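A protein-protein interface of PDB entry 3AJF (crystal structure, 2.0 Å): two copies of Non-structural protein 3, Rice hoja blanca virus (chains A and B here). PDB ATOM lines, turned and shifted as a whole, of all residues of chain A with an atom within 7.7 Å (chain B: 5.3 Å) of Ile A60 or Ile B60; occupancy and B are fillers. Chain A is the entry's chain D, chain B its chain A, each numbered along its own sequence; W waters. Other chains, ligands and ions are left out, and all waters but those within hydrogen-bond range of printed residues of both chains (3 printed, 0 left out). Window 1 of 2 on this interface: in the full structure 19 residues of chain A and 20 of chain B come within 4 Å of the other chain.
The backbone carbonyl oxygen of Phe B88 is in hydrogen-bond range of the guanidinium group of Arg A74 (2.9 Å).
O of Ile B60 sits at hydrogen-bond distance from OG of Ser B64, 2.8 Å away.
The side-chain hydroxyl (OG) of Ser A64 sits at hydrogen-bond distance from the backbone carbonyl oxygen (O) of Ile A60 (2.9 Å).
The backbone carbonyl oxygen (O) of Val A81 sits close to the side-chain hydroxyl (OG) of Ser A85 (3.5 Å).
The backbone carbonyl oxygen (O) of Leu A63 is in hydrogen-bond range of the guanidinium group (NH2) of Arg A74.
OG of Ser A64 sits at hydrogen-bond distance from ND1 of His A65, 2.8 Å away.
Ser B64 touches Pro A49 (CB to O, 3.7 Å).
Glu A50 touches His B65 (OE2 to CE1, 3.9 Å).
CB of Ser A53 touches OG of Ser B64 (3.7 Å).
OG of Ser B53 touches CG2 of Ile A60, at 3.8 Å.
CD1 of Ile B60 touches CD1 of Ile A60, at 3.5 Å.
Ser A64 touches Ser B53.
Ser A64 touches Phe B88 (CB to CE1, 3.7 Å).
CB of Ser A85 touches CG1 of Val B81, 3.7 Å away.
Phe A88 touches Leu B63.
Ser B64 touches Phe A88.
Ile A60 touches just these residues of chain B: Ser B53 (3.8 Å) and Ile B60 (3.5 Å).
Of the printed residues of chain A, Ile B60 touches Ser A53 and Ile A60.
Of the printed residues of chain B, Phe A88 touches Leu B63 (3.8 Å) and Ser B64 (3.7 Å).
Printed residues of chain A within 4 Å of Leu B63: Phe A88 (3.8 Å).
Along chain B the printed residues that touch a printed residue of chain A span positions 53 to 88.
Ser A53 touches Ile B60, and with the chains exchanged Ile A60 touches Ser B53.
Ser A53 touches Ser B64, and with the chains exchanged Ser A64 touches Ser B53.
Ile B60 touches its own counterpart, Ile A60.
Ser A64 touches Phe B88, and with the chains exchanged Phe A88 touches Ser B64.
Water W3 lies within hydrogen-bond range of OG of Ser B53 and OG of Ser A64.
Water W1 lies within hydrogen-bond range of OG of Ser A53 and OG of Ser B64.
Water W2 lies within hydrogen-bond range of the backbone carbonyl oxygen of Ser B64 (2.7 Å) and the side-chain carboxylate of Glu A50 (2.9 Å).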
ATOM      1  N   PHE A  23      18.209   3.538 -20.558  1.00  0.00           N
ATOM      2  CA  PHE A  23      19.393   2.808 -20.113  1.00  0.00           C
ATOM      3  C   PHE A  23      19.770   1.743 -21.152  1.00  0.00           C
ATOM      4  O   PHE A  23      20.920   1.696 -21.606  1.00  0.00           O
ATOM      5  CB  PHE A  23      19.078   2.221 -18.734  1.00  0.00           C
ATOM      6  CG  PHE A  23      20.182   1.350 -18.104  1.00  0.00           C
ATOM      7  CD1 PHE A  23      21.497   1.337 -18.544  1.00  0.00           C
ATOM      8  CD2 PHE A  23      19.853   0.562 -17.011  1.00  0.00           C
ATOM      9  CE1 PHE A  23      22.476   0.517 -17.915  1.00  0.00           C
ATOM     10  CE2 PHE A  23      20.819  -0.262 -16.356  1.00  0.00           C
ATOM     11  CZ  PHE A  23      22.144  -0.275 -16.819  1.00  0.00           C
ATOM     12  N   PRO A  49      30.220 -11.945 -14.827  1.00  0.00           N
ATOM     13  CA  PRO A  49      30.791 -10.753 -14.209  1.00  0.00           C
ATOM     14  C   PRO A  49      31.183  -9.685 -15.217  1.00  0.00           C
ATOM     15  O   PRO A  49      31.067  -8.498 -14.918  1.00  0.00           O
ATOM     16  CB  PRO A  49      32.024 -11.290 -13.478  1.00  0.00           C
ATOM     17  CG  PRO A  49      32.414 -12.514 -14.267  1.00  0.00           C
ATOM     18  CD  PRO A  49      31.111 -13.117 -14.686  1.00  0.00           C
ATOM     19  N   GLU A  50      31.661 -10.077 -16.389  1.00  0.00           N
ATOM     20  CA  GLU A  50      32.019  -9.068 -17.376  1.00  0.00           C
ATOM     21  C   GLU A  50      30.789  -8.343 -17.903  1.00  0.00           C
ATOM     22  O   GLU A  50      30.835  -7.148 -18.090  1.00  0.00           O
ATOM     23  CB  GLU A  50      32.836  -9.678 -18.521  1.00  0.00           C
ATOM     24  CG  GLU A  50      34.096 -10.328 -17.971  1.00  0.00           C
ATOM     25  CD  GLU A  50      35.063 -10.846 -19.030  1.00  0.00           C
ATOM     26  OE1 GLU A  50      34.634 -11.149 -20.184  1.00  0.00           O
ATOM     27  OE2 GLU A  50      36.264 -10.960 -18.671  1.00  0.00           O
ATOM     28  N   LEU A  52      27.951  -7.948 -16.282  1.00  0.00           N
ATOM     29  CA  LEU A  52      27.482  -7.134 -15.190  1.00  0.00           C
ATOM     30  C   LEU A  52      28.301  -5.855 -15.143  1.00  0.00           C
ATOM     31  O   LEU A  52      27.743  -4.770 -15.015  1.00  0.00           O
ATOM     32  CB  LEU A  52      27.575  -7.894 -13.847  1.00  0.00           C
ATOM     33  CG  LEU A  52      27.046  -7.063 -12.657  1.00  0.00           C
ATOM     34  CD1 LEU A  52      25.605  -6.449 -12.840  1.00  0.00           C
ATOM     35  CD2 LEU A  52      27.139  -7.850 -11.339  1.00  0.00           C
ATOM     36  N   SER A  53      29.618  -5.988 -15.308  1.00  0.00           N
ATOM     37  CA  SER A  53      30.514  -4.854 -15.274  1.00  0.00           C
ATOM     38  C   SER A  53      30.115  -3.811 -16.320  1.00  0.00           C
ATOM     39  O   SER A  53      29.960  -2.628 -15.991  1.00  0.00           O
ATOM     40  CB  SER A  53      31.957  -5.300 -15.563  1.00  0.00           C
ATOM     41  OG  SER A  53      32.715  -4.123 -15.751  1.00  0.00           O
ATOM     42  N   VAL A  54      29.955  -4.231 -17.573  1.00  0.00           N
ATOM     43  CA  VAL A  54      29.566  -3.265 -18.613  1.00  0.00           C
ATOM     44  C   VAL A  54      28.178  -2.608 -18.394  1.00  0.00           C
ATOM     45  O   VAL A  54      28.060  -1.432 -18.638  1.00  0.00           O
ATOM     46  CB  VAL A  54      29.804  -3.708 -20.094  1.00  0.00           C
ATOM     47  CG1 VAL A  54      31.070  -4.651 -20.261  1.00  0.00           C
ATOM     48  CG2 VAL A  54      28.577  -4.236 -20.723  1.00  0.00           C
ATOM     49  N   PHE A  55      27.177  -3.400 -17.980  1.00  0.00           N
ATOM     50  CA  PHE A  55      25.848  -2.937 -17.522  1.00  0.00           C
ATOM     51  C   PHE A  55      25.969  -1.817 -16.464  1.00  0.00           C
ATOM     52  O   PHE A  55      25.393  -0.712 -16.616  1.00  0.00           O
ATOM     53  CB  PHE A  55      25.098  -4.187 -17.020  1.00  0.00           C
ATOM     54  CG  PHE A  55      23.739  -3.949 -16.384  1.00  0.00           C
ATOM     55  CD1 PHE A  55      22.566  -3.983 -17.157  1.00  0.00           C
ATOM     56  CD2 PHE A  55      23.617  -3.832 -14.996  1.00  0.00           C
ATOM     57  CE1 PHE A  55      21.275  -3.833 -16.552  1.00  0.00           C
ATOM     58  CE2 PHE A  55      22.326  -3.678 -14.374  1.00  0.00           C
ATOM     59  CZ  PHE A  55      21.162  -3.683 -15.173  1.00  0.00           C
ATOM     60  N   LEU A  56      26.710  -2.082 -15.394  1.00  0.00           N
ATOM     61  CA  LEU A  56      26.872  -1.079 -14.338  1.00  0.00           C
ATOM     62  C   LEU A  56      27.623   0.151 -14.814  1.00  0.00           C
ATOM     63  O   LEU A  56      27.307   1.265 -14.428  1.00  0.00           O
ATOM     64  CB  LEU A  56      27.608  -1.682 -13.139  1.00  0.00           C
ATOM     65  CG  LEU A  56      26.817  -2.763 -12.390  1.00  0.00           C
ATOM     66  CD1 LEU A  56      27.690  -3.314 -11.235  1.00  0.00           C
ATOM     67  CD2 LEU A  56      25.533  -2.196 -11.838  1.00  0.00           C
ATOM     68  N   LYS A  57      28.647  -0.048 -15.637  1.00  0.00           N
ATOM     69  CA  LYS A  57      29.431   1.058 -16.113  1.00  0.00           C
ATOM     70  C   LYS A  57      28.620   2.051 -16.991  1.00  0.00           C
ATOM     71  O   LYS A  57      28.900   3.242 -16.952  1.00  0.00           O
ATOM     72  CB  LYS A  57      30.690   0.538 -16.852  1.00  0.00           C
ATOM     73  CG  LYS A  57      31.796   0.061 -15.917  1.00  0.00           C
ATOM     74  CD  LYS A  57      32.838  -0.815 -16.640  1.00  0.00           C
ATOM     75  CE  LYS A  57      33.921  -0.057 -17.311  1.00  0.00           C
ATOM     76  NZ  LYS A  57      34.673  -1.020 -18.178  1.00  0.00           N
ATOM     77  N   SER A  58      27.647   1.562 -17.778  1.00  0.00           N
ATOM     78  CA  SER A  58      26.782   2.453 -18.572  1.00  0.00           C
ATOM     79  C   SER A  58      25.893   3.257 -17.622  1.00  0.00           C
ATOM     80  O   SER A  58      25.705   4.451 -17.816  1.00  0.00           O
ATOM     81  CB  SER A  58      25.919   1.689 -19.620  1.00  0.00           C
ATOM     82  OG  SER A  58      26.643   1.501 -20.854  1.00  0.00           O
ATOM     83  N   ALA A  59      25.329   2.601 -16.609  1.00  0.00           N
ATOM     84  CA  ALA A  59      24.499   3.320 -15.633  1.00  0.00           C
ATOM     85  C   ALA A  59      25.317   4.388 -14.931  1.00  0.00           C
ATOM     86  O   ALA A  59      24.810   5.474 -14.673  1.00  0.00           O
ATOM     87  CB  ALA A  59      23.887   2.368 -14.629  1.00  0.00           C
ATOM     88  N   ILE A  60      26.575   4.068 -14.626  1.00  0.00           N
ATOM     89  CA  ILE A  60      27.453   5.008 -13.908  1.00  0.00           C
ATOM     90  C   ILE A  60      27.820   6.176 -14.803  1.00  0.00           C
ATOM     91  O   ILE A  60      27.767   7.307 -14.353  1.00  0.00           O
ATOM     92  CB  ILE A  60      28.681   4.313 -13.294  1.00  0.00           C
ATOM     93  CG1 ILE A  60      28.250   3.568 -12.035  1.00  0.00           C
ATOM     94  CG2 ILE A  60      29.764   5.291 -12.912  1.00  0.00           C
ATOM     95  CD1 ILE A  60      29.277   2.467 -11.594  1.00  0.00           C
ATOM     96  N   TRP A  61      28.165   5.905 -16.060  1.00  0.00           N
ATOM     97  CA  TRP A  61      28.388   6.978 -17.017  1.00  0.00           C
ATOM     98  C   TRP A  61      27.173   7.921 -17.085  1.00  0.00           C
ATOM     99  O   TRP A  61      27.332   9.145 -17.053  1.00  0.00           O
ATOM    100  CB  TRP A  61      28.725   6.405 -18.400  1.00  0.00           C
ATOM    101  CG  TRP A  61      28.848   7.504 -19.403  1.00  0.00           C
ATOM    102  CD1 TRP A  61      29.972   8.245 -19.712  1.00  0.00           C
ATOM    103  CD2 TRP A  61      27.782   8.014 -20.194  1.00  0.00           C
ATOM    104  NE1 TRP A  61      29.645   9.170 -20.702  1.00  0.00           N
ATOM    105  CE2 TRP A  61      28.307   9.047 -20.996  1.00  0.00           C
ATOM    106  CE3 TRP A  61      26.432   7.662 -20.329  1.00  0.00           C
ATOM    107  CZ2 TRP A  61      27.530   9.746 -21.895  1.00  0.00           C
ATOM    108  CZ3 TRP A  61      25.650   8.370 -21.226  1.00  0.00           C
ATOM    109  CH2 TRP A  61      26.208   9.395 -22.010  1.00  0.00           C
ATOM    110  N   MET A  62      25.964   7.350 -17.150  1.00  0.00           N
ATOM    111  CA  MET A  62      24.744   8.160 -17.220  1.00  0.00           C
ATOM    112  C   MET A  62      24.625   9.094 -16.011  1.00  0.00           C
ATOM    113  O   MET A  62      24.141  10.220 -16.133  1.00  0.00           O
ATOM    114  CB  MET A  62      23.507   7.270 -17.292  1.00  0.00           C
ATOM    115  CG  MET A  62      23.383   6.452 -18.583  1.00  0.00           C
ATOM    116  SD  MET A  62      21.960   5.090 -18.458  1.00  0.00           S
ATOM    117  CE  MET A  62      20.346   6.211 -18.429  1.00  0.00           C
ATOM    118  N   LEU A  63      25.034   8.598 -14.845  1.00  0.00           N
ATOM    119  CA  LEU A  63      24.929   9.356 -13.609  1.00  0.00           C
ATOM    120  C   LEU A  63      26.096  10.334 -13.448  1.00  0.00           C
ATOM    121  O   LEU A  63      25.950  11.367 -12.782  1.00  0.00           O
ATOM    122  CB  LEU A  63      24.914   8.399 -12.391  1.00  0.00           C
ATOM    123  CG  LEU A  63      23.662   7.526 -12.124  1.00  0.00           C
ATOM    124  CD1 LEU A  63      23.954   6.448 -11.080  1.00  0.00           C
ATOM    125  CD2 LEU A  63      22.468   8.387 -11.673  1.00  0.00           C
ATOM    126  N   SER A  64      27.256  10.011 -14.019  1.00  0.00           N
ATOM    127  CA  SER A  64      28.451  10.836 -13.792  1.00  0.00           C
ATOM    128  C   SER A  64      28.797  11.803 -14.906  1.00  0.00           C
ATOM    129  O   SER A  64      29.457  12.803 -14.633  1.00  0.00           O
ATOM    130  CB  SER A  64      29.655   9.949 -13.459  1.00  0.00           C
ATOM    131  OG  SER A  64      29.984   9.126 -14.592  1.00  0.00           O
ATOM    132  N   HIS A  65      28.302  11.562 -16.132  1.00  0.00           N
ATOM    133  CA  HIS A  65      28.683  12.401 -17.295  1.00  0.00           C
ATOM    134  C   HIS A  65      27.531  13.025 -18.032  1.00  0.00           C
ATOM    135  O   HIS A  65      27.683  14.113 -18.564  1.00  0.00           O
ATOM    136  CB  HIS A  65      29.483  11.592 -18.324  1.00  0.00           C
ATOM    137  CG  HIS A  65      30.868  11.256 -17.884  1.00  0.00           C
ATOM    138  ND1 HIS A  65      31.134  10.454 -16.802  1.00  0.00           N
ATOM    139  CD2 HIS A  65      32.071  11.631 -18.378  1.00  0.00           C
ATOM    140  CE1 HIS A  65      32.440  10.325 -16.654  1.00  0.00           C
ATOM    141  NE2 HIS A  65      33.033  11.035 -17.597  1.00  0.00           N
ATOM    142  N   LYS A  66      26.399  12.339 -18.091  1.00  0.00           N
ATOM    143  CA  LYS A  66      25.287  12.730 -18.946  1.00  0.00           C
ATOM    144  C   LYS A  66      24.600  13.919 -18.318  1.00  0.00           C
ATOM    145  O   LYS A  66      23.967  13.810 -17.271  1.00  0.00           O
ATOM    146  CB  LYS A  66      24.318  11.555 -19.124  1.00  0.00           C
ATOM    147  CG  LYS A  66      23.136  11.849 -20.040  1.00  0.00           C
ATOM    148  CD  LYS A  66      22.321  10.576 -20.303  1.00  0.00           C
ATOM    149  CE  LYS A  66      21.074  10.905 -21.071  1.00  0.00           C
ATOM    150  NZ  LYS A  66      21.406  11.443 -22.460  1.00  0.00           N
ATOM    151  N   ARG A  74      17.392  10.074 -11.394  1.00  0.00           N
ATOM    152  CA  ARG A  74      18.612   9.919 -10.589  1.00  0.00           C
ATOM    153  C   ARG A  74      18.463   8.889  -9.463  1.00  0.00           C
ATOM    154  O   ARG A  74      19.296   8.007  -9.346  1.00  0.00           O
ATOM    155  CB  ARG A  74      19.143  11.240 -10.040  1.00  0.00           C
ATOM    156  CG  ARG A  74      19.613  12.215 -11.113  1.00  0.00           C
ATOM    157  CD  ARG A  74      20.502  13.317 -10.498  1.00  0.00           C
ATOM    158  NE  ARG A  74      21.832  12.758 -10.228  1.00  0.00           N
ATOM    159  CZ  ARG A  74      22.729  12.488 -11.188  1.00  0.00           C
ATOM    160  NH1 ARG A  74      22.453  12.735 -12.469  1.00  0.00           N
ATOM    161  NH2 ARG A  74      23.901  11.967 -10.877  1.00  0.00           N
ATOM    162  N   LEU A  77      17.804   5.201 -10.864  1.00  0.00           N
ATOM    163  CA  LEU A  77      18.995   4.714 -11.566  1.00  0.00           C
ATOM    164  C   LEU A  77      20.109   4.390 -10.566  1.00  0.00           C
ATOM    165  O   LEU A  77      20.798   3.389 -10.703  1.00  0.00           O
ATOM    166  CB  LEU A  77      19.511   5.686 -12.652  1.00  0.00           C
ATOM    167  CG  LEU A  77      20.690   5.232 -13.550  1.00  0.00           C
ATOM    168  CD1 LEU A  77      20.386   3.854 -14.200  1.00  0.00           C
ATOM    169  CD2 LEU A  77      20.957   6.251 -14.646  1.00  0.00           C
ATOM    170  N   VAL A  81      22.006   0.736  -9.743  1.00  0.00           N
ATOM    171  CA  VAL A  81      23.457   0.511  -9.532  1.00  0.00           C
ATOM    172  C   VAL A  81      23.792  -0.186  -8.196  1.00  0.00           C
ATOM    173  O   VAL A  81      24.494  -1.172  -8.190  1.00  0.00           O
ATOM    174  CB  VAL A  81      24.295   1.803  -9.708  1.00  0.00           C
ATOM    175  CG1 VAL A  81      25.735   1.597  -9.297  1.00  0.00           C
ATOM    176  CG2 VAL A  81      24.177   2.301 -11.142  1.00  0.00           C
ATOM    177  N   SER A  85      24.965  -4.153  -8.206  1.00  0.00           N
ATOM    178  CA  SER A  85      26.352  -4.370  -7.788  1.00  0.00           C
ATOM    179  C   SER A  85      26.486  -5.491  -6.739  1.00  0.00           C
ATOM    180  O   SER A  85      27.506  -6.159  -6.679  1.00  0.00           O
ATOM    181  CB  SER A  85      27.019  -3.048  -7.364  1.00  0.00           C
ATOM    182  OG  SER A  85      26.663  -2.808  -6.012  1.00  0.00           O
ATOM    183  N   PHE A  88      27.961  -9.144  -7.321  1.00  0.00           N
ATOM    184  CA  PHE A  88      29.403  -9.434  -7.364  1.00  0.00           C
ATOM    185  C   PHE A  88      29.900 -10.260  -6.176  1.00  0.00           C
ATOM    186  O   PHE A  88      30.987 -10.833  -6.240  1.00  0.00           O
ATOM    187  CB  PHE A  88      30.293  -8.174  -7.484  1.00  0.00           C
ATOM    188  CG  PHE A  88      30.405  -7.629  -8.890  1.00  0.00           C
ATOM    189  CD1 PHE A  88      30.842  -8.435  -9.940  1.00  0.00           C
ATOM    190  CD2 PHE A  88      30.090  -6.310  -9.158  1.00  0.00           C
ATOM    191  CE1 PHE A  88      30.959  -7.938 -11.229  1.00  0.00           C
ATOM    192  CE2 PHE A  88      30.198  -5.802 -10.475  1.00  0.00           C
ATOM    193  CZ  PHE A  88      30.635  -6.622 -11.500  1.00  0.00           C
ATOM    194  N   SER B  53      33.187   8.370 -10.200  1.00  0.00           N
ATOM    195  CA  SER B  53      33.080   7.414 -11.306  1.00  0.00           C
ATOM    196  C   SER B  53      34.336   6.573 -11.446  1.00  0.00           C
ATOM    197  O   SER B  53      34.266   5.336 -11.582  1.00  0.00           O
ATOM    198  CB  SER B  53      32.840   8.149 -12.626  1.00  0.00           C
ATOM    199  OG  SER B  53      32.902   7.227 -13.695  1.00  0.00           O
ATOM    200  N   LEU B  56      34.739   4.220  -8.303  1.00  0.00           N
ATOM    201  CA  LEU B  56      33.856   3.043  -8.431  1.00  0.00           C
ATOM    202  C   LEU B  56      34.291   2.071  -9.533  1.00  0.00           C
ATOM    203  O   LEU B  56      34.190   0.841  -9.369  1.00  0.00           O
ATOM    204  CB  LEU B  56      32.396   3.457  -8.656  1.00  0.00           C
ATOM    205  CG  LEU B  56      31.727   4.267  -7.527  1.00  0.00           C
ATOM    206  CD1 LEU B  56      30.434   4.831  -8.079  1.00  0.00           C
ATOM    207  CD2 LEU B  56      31.445   3.439  -6.336  1.00  0.00           C
ATOM    208  N   LYS B  57      34.746   2.613 -10.664  1.00  0.00           N
ATOM    209  CA  LYS B  57      35.176   1.774 -11.774  1.00  0.00           C
ATOM    210  C   LYS B  57      36.390   0.905 -11.432  1.00  0.00           C
ATOM    211  O   LYS B  57      36.487  -0.240 -11.906  1.00  0.00           O
ATOM    212  CB  LYS B  57      35.462   2.619 -13.009  1.00  0.00           C
ATOM    213  CG  LYS B  57      34.220   3.026 -13.729  1.00  0.00           C
ATOM    214  CD  LYS B  57      34.441   4.334 -14.465  1.00  0.00           C
ATOM    215  CE  LYS B  57      34.875   4.174 -15.885  1.00  0.00           C
ATOM    216  NZ  LYS B  57      35.392   5.537 -16.314  1.00  0.00           N
ATOM    217  N   SER B  58      37.300   1.422 -10.610  1.00  0.00           N
ATOM    218  CA  SER B  58      38.428   0.594 -10.118  1.00  0.00           C
ATOM    219  C   SER B  58      37.948  -0.556  -9.223  1.00  0.00           C
ATOM    220  O   SER B  58      38.430  -1.701  -9.351  1.00  0.00           O
ATOM    221  CB  SER B  58      39.491   1.421  -9.385  1.00  0.00           C
ATOM    222  OG  SER B  58      40.472   1.939 -10.269  1.00  0.00           O
ATOM    223  N   ALA B  59      37.024  -0.257  -8.311  1.00  0.00           N
ATOM    224  CA  ALA B  59      36.447  -1.292  -7.434  1.00  0.00           C
ATOM    225  C   ALA B  59      35.665  -2.349  -8.233  1.00  0.00           C
ATOM    226  O   ALA B  59      35.765  -3.526  -7.954  1.00  0.00           O
ATOM    227  CB  ALA B  59      35.580  -0.638  -6.341  1.00  0.00           C
ATOM    228  N   ILE B  60      34.886  -1.918  -9.227  1.00  0.00           N
ATOM    229  CA  ILE B  60      34.135  -2.818 -10.119  1.00  0.00           C
ATOM    230  C   ILE B  60      35.101  -3.681 -10.967  1.00  0.00           C
ATOM    231  O   ILE B  60      34.893  -4.884 -11.130  1.00  0.00           O
ATOM    232  CB  ILE B  60      33.136  -2.049 -11.005  1.00  0.00           C
ATOM    233  CG1 ILE B  60      32.010  -1.449 -10.096  1.00  0.00           C
ATOM    234  CG2 ILE B  60      32.530  -2.985 -12.112  1.00  0.00           C
ATOM    235  CD1 ILE B  60      31.053  -0.418 -10.807  1.00  0.00           C
ATOM    236  N   TRP B  61      36.166  -3.066 -11.470  1.00  0.00           N
ATOM    237  CA  TRP B  61      37.219  -3.842 -12.145  1.00  0.00           C
ATOM    238  C   TRP B  61      37.793  -4.965 -11.259  1.00  0.00           C
ATOM    239  O   TRP B  61      37.926  -6.112 -11.707  1.00  0.00           O
ATOM    240  CB  TRP B  61      38.332  -2.951 -12.734  1.00  0.00           C
ATOM    241  CG  TRP B  61      39.421  -3.813 -13.291  1.00  0.00           C
ATOM    242  CD1 TRP B  61      39.524  -4.300 -14.578  1.00  0.00           C
ATOM    243  CD2 TRP B  61      40.533  -4.320 -12.574  1.00  0.00           C
ATOM    244  NE1 TRP B  61      40.670  -5.072 -14.697  1.00  0.00           N
ATOM    245  CE2 TRP B  61      41.294  -5.115 -13.474  1.00  0.00           C
ATOM    246  CE3 TRP B  61      40.987  -4.167 -11.255  1.00  0.00           C
ATOM    247  CZ2 TRP B  61      42.473  -5.767 -13.090  1.00  0.00           C
ATOM    248  CZ3 TRP B  61      42.180  -4.817 -10.872  1.00  0.00           C
ATOM    249  CH2 TRP B  61      42.897  -5.619 -11.791  1.00  0.00           C
ATOM    250  N   MET B  62      38.117  -4.644 -10.010  1.00  0.00           N
ATOM    251  CA  MET B  62      38.652  -5.620  -9.055  1.00  0.00           C
ATOM    252  C   MET B  62      37.690  -6.793  -8.829  1.00  0.00           C
ATOM    253  O   MET B  62      38.135  -7.927  -8.581  1.00  0.00           O
ATOM    254  CB  MET B  62      38.951  -4.966  -7.710  1.00  0.00           C
ATOM    255  CG  MET B  62      40.078  -3.947  -7.700  1.00  0.00           C
ATOM    256  SD  MET B  62      40.151  -2.796  -6.100  1.00  0.00           S
ATOM    257  CE  MET B  62      40.629  -4.050  -4.614  1.00  0.00           C
ATOM    258  N   LEU B  63      36.380  -6.520  -8.847  1.00  0.00           N
ATOM    259  CA  LEU B  63      35.376  -7.571  -8.641  1.00  0.00           C
ATOM    260  C   LEU B  63      35.091  -8.379  -9.912  1.00  0.00           C
ATOM    261  O   LEU B  63      34.726  -9.560  -9.839  1.00  0.00           O
ATOM    262  CB  LEU B  63      34.064  -6.963  -8.129  1.00  0.00           C
ATOM    263  CG  LEU B  63      34.121  -6.403  -6.708  1.00  0.00           C
ATOM    264  CD1 LEU B  63      32.958  -5.410  -6.410  1.00  0.00           C
ATOM    265  CD2 LEU B  63      34.129  -7.589  -5.736  1.00  0.00           C
ATOM    266  N   SER B  64      35.205  -7.736 -11.060  1.00  0.00           N
ATOM    267  CA  SER B  64      34.766  -8.350 -12.303  1.00  0.00           C
ATOM    268  C   SER B  64      35.917  -9.009 -13.058  1.00  0.00           C
ATOM    269  O   SER B  64      35.682  -9.911 -13.867  1.00  0.00           O
ATOM    270  CB  SER B  64      34.068  -7.313 -13.186  1.00  0.00           C
ATOM    271  OG  SER B  64      34.955  -6.274 -13.599  1.00  0.00           O
ATOM    272  N   HIS B  65      37.147  -8.543 -12.824  1.00  0.00           N
ATOM    273  CA  HIS B  65      38.288  -8.987 -13.663  1.00  0.00           C
ATOM    274  C   HIS B  65      39.434  -9.603 -12.870  1.00  0.00           C
ATOM    275  O   HIS B  65      40.128 -10.476 -13.381  1.00  0.00           O
ATOM    276  CB  HIS B  65      38.839  -7.851 -14.522  1.00  0.00           C
ATOM    277  CG  HIS B  65      37.921  -7.420 -15.618  1.00  0.00           C
ATOM    278  ND1 HIS B  65      38.039  -7.867 -16.914  1.00  0.00           N
ATOM    279  CD2 HIS B  65      36.863  -6.582 -15.606  1.00  0.00           C
ATOM    280  CE1 HIS B  65      37.082  -7.334 -17.655  1.00  0.00           C
ATOM    281  NE2 HIS B  65      36.362  -6.540 -16.883  1.00  0.00           N
ATOM    282  N   VAL B  81      31.184  -0.516  -3.093  1.00  0.00           N
ATOM    283  CA  VAL B  81      30.618  -0.132  -4.374  1.00  0.00           C
ATOM    284  C   VAL B  81      29.162   0.307  -4.189  1.00  0.00           C
ATOM    285  O   VAL B  81      28.740   1.373  -4.671  1.00  0.00           O
ATOM    286  CB  VAL B  81      30.731  -1.244  -5.462  1.00  0.00           C
ATOM    287  CG1 VAL B  81      29.873  -0.869  -6.685  1.00  0.00           C
ATOM    288  CG2 VAL B  81      32.109  -1.362  -5.899  1.00  0.00           C
ATOM    289  N   PHE B  88      25.587   9.404  -5.961  1.00  0.00           N
ATOM    290  CA  PHE B  88      25.107   9.928  -7.247  1.00  0.00           C
ATOM    291  C   PHE B  88      23.718  10.552  -7.222  1.00  0.00           C
ATOM    292  O   PHE B  88      23.357  11.293  -8.158  1.00  0.00           O
ATOM    293  CB  PHE B  88      25.151   8.879  -8.356  1.00  0.00           C
ATOM    294  CG  PHE B  88      26.538   8.681  -8.935  1.00  0.00           C
ATOM    295  CD1 PHE B  88      27.271   9.771  -9.389  1.00  0.00           C
ATOM    296  CD2 PHE B  88      27.087   7.412  -9.036  1.00  0.00           C
ATOM    297  CE1 PHE B  88      28.524   9.599  -9.969  1.00  0.00           C
ATOM    298  CE2 PHE B  88      28.365   7.238  -9.593  1.00  0.00           C
ATOM    299  CZ  PHE B  88      29.075   8.349 -10.053  1.00  0.00           C
HETATM  300  O   HOH W   1      35.153  -3.667 -14.902  1.00  0.00           O
HETATM  301  O   HOH W   2      36.304 -11.597 -15.892  1.00  0.00           O
HETATM  302  O   HOH W   3      31.563   6.867 -15.795  1.00  0.00           O
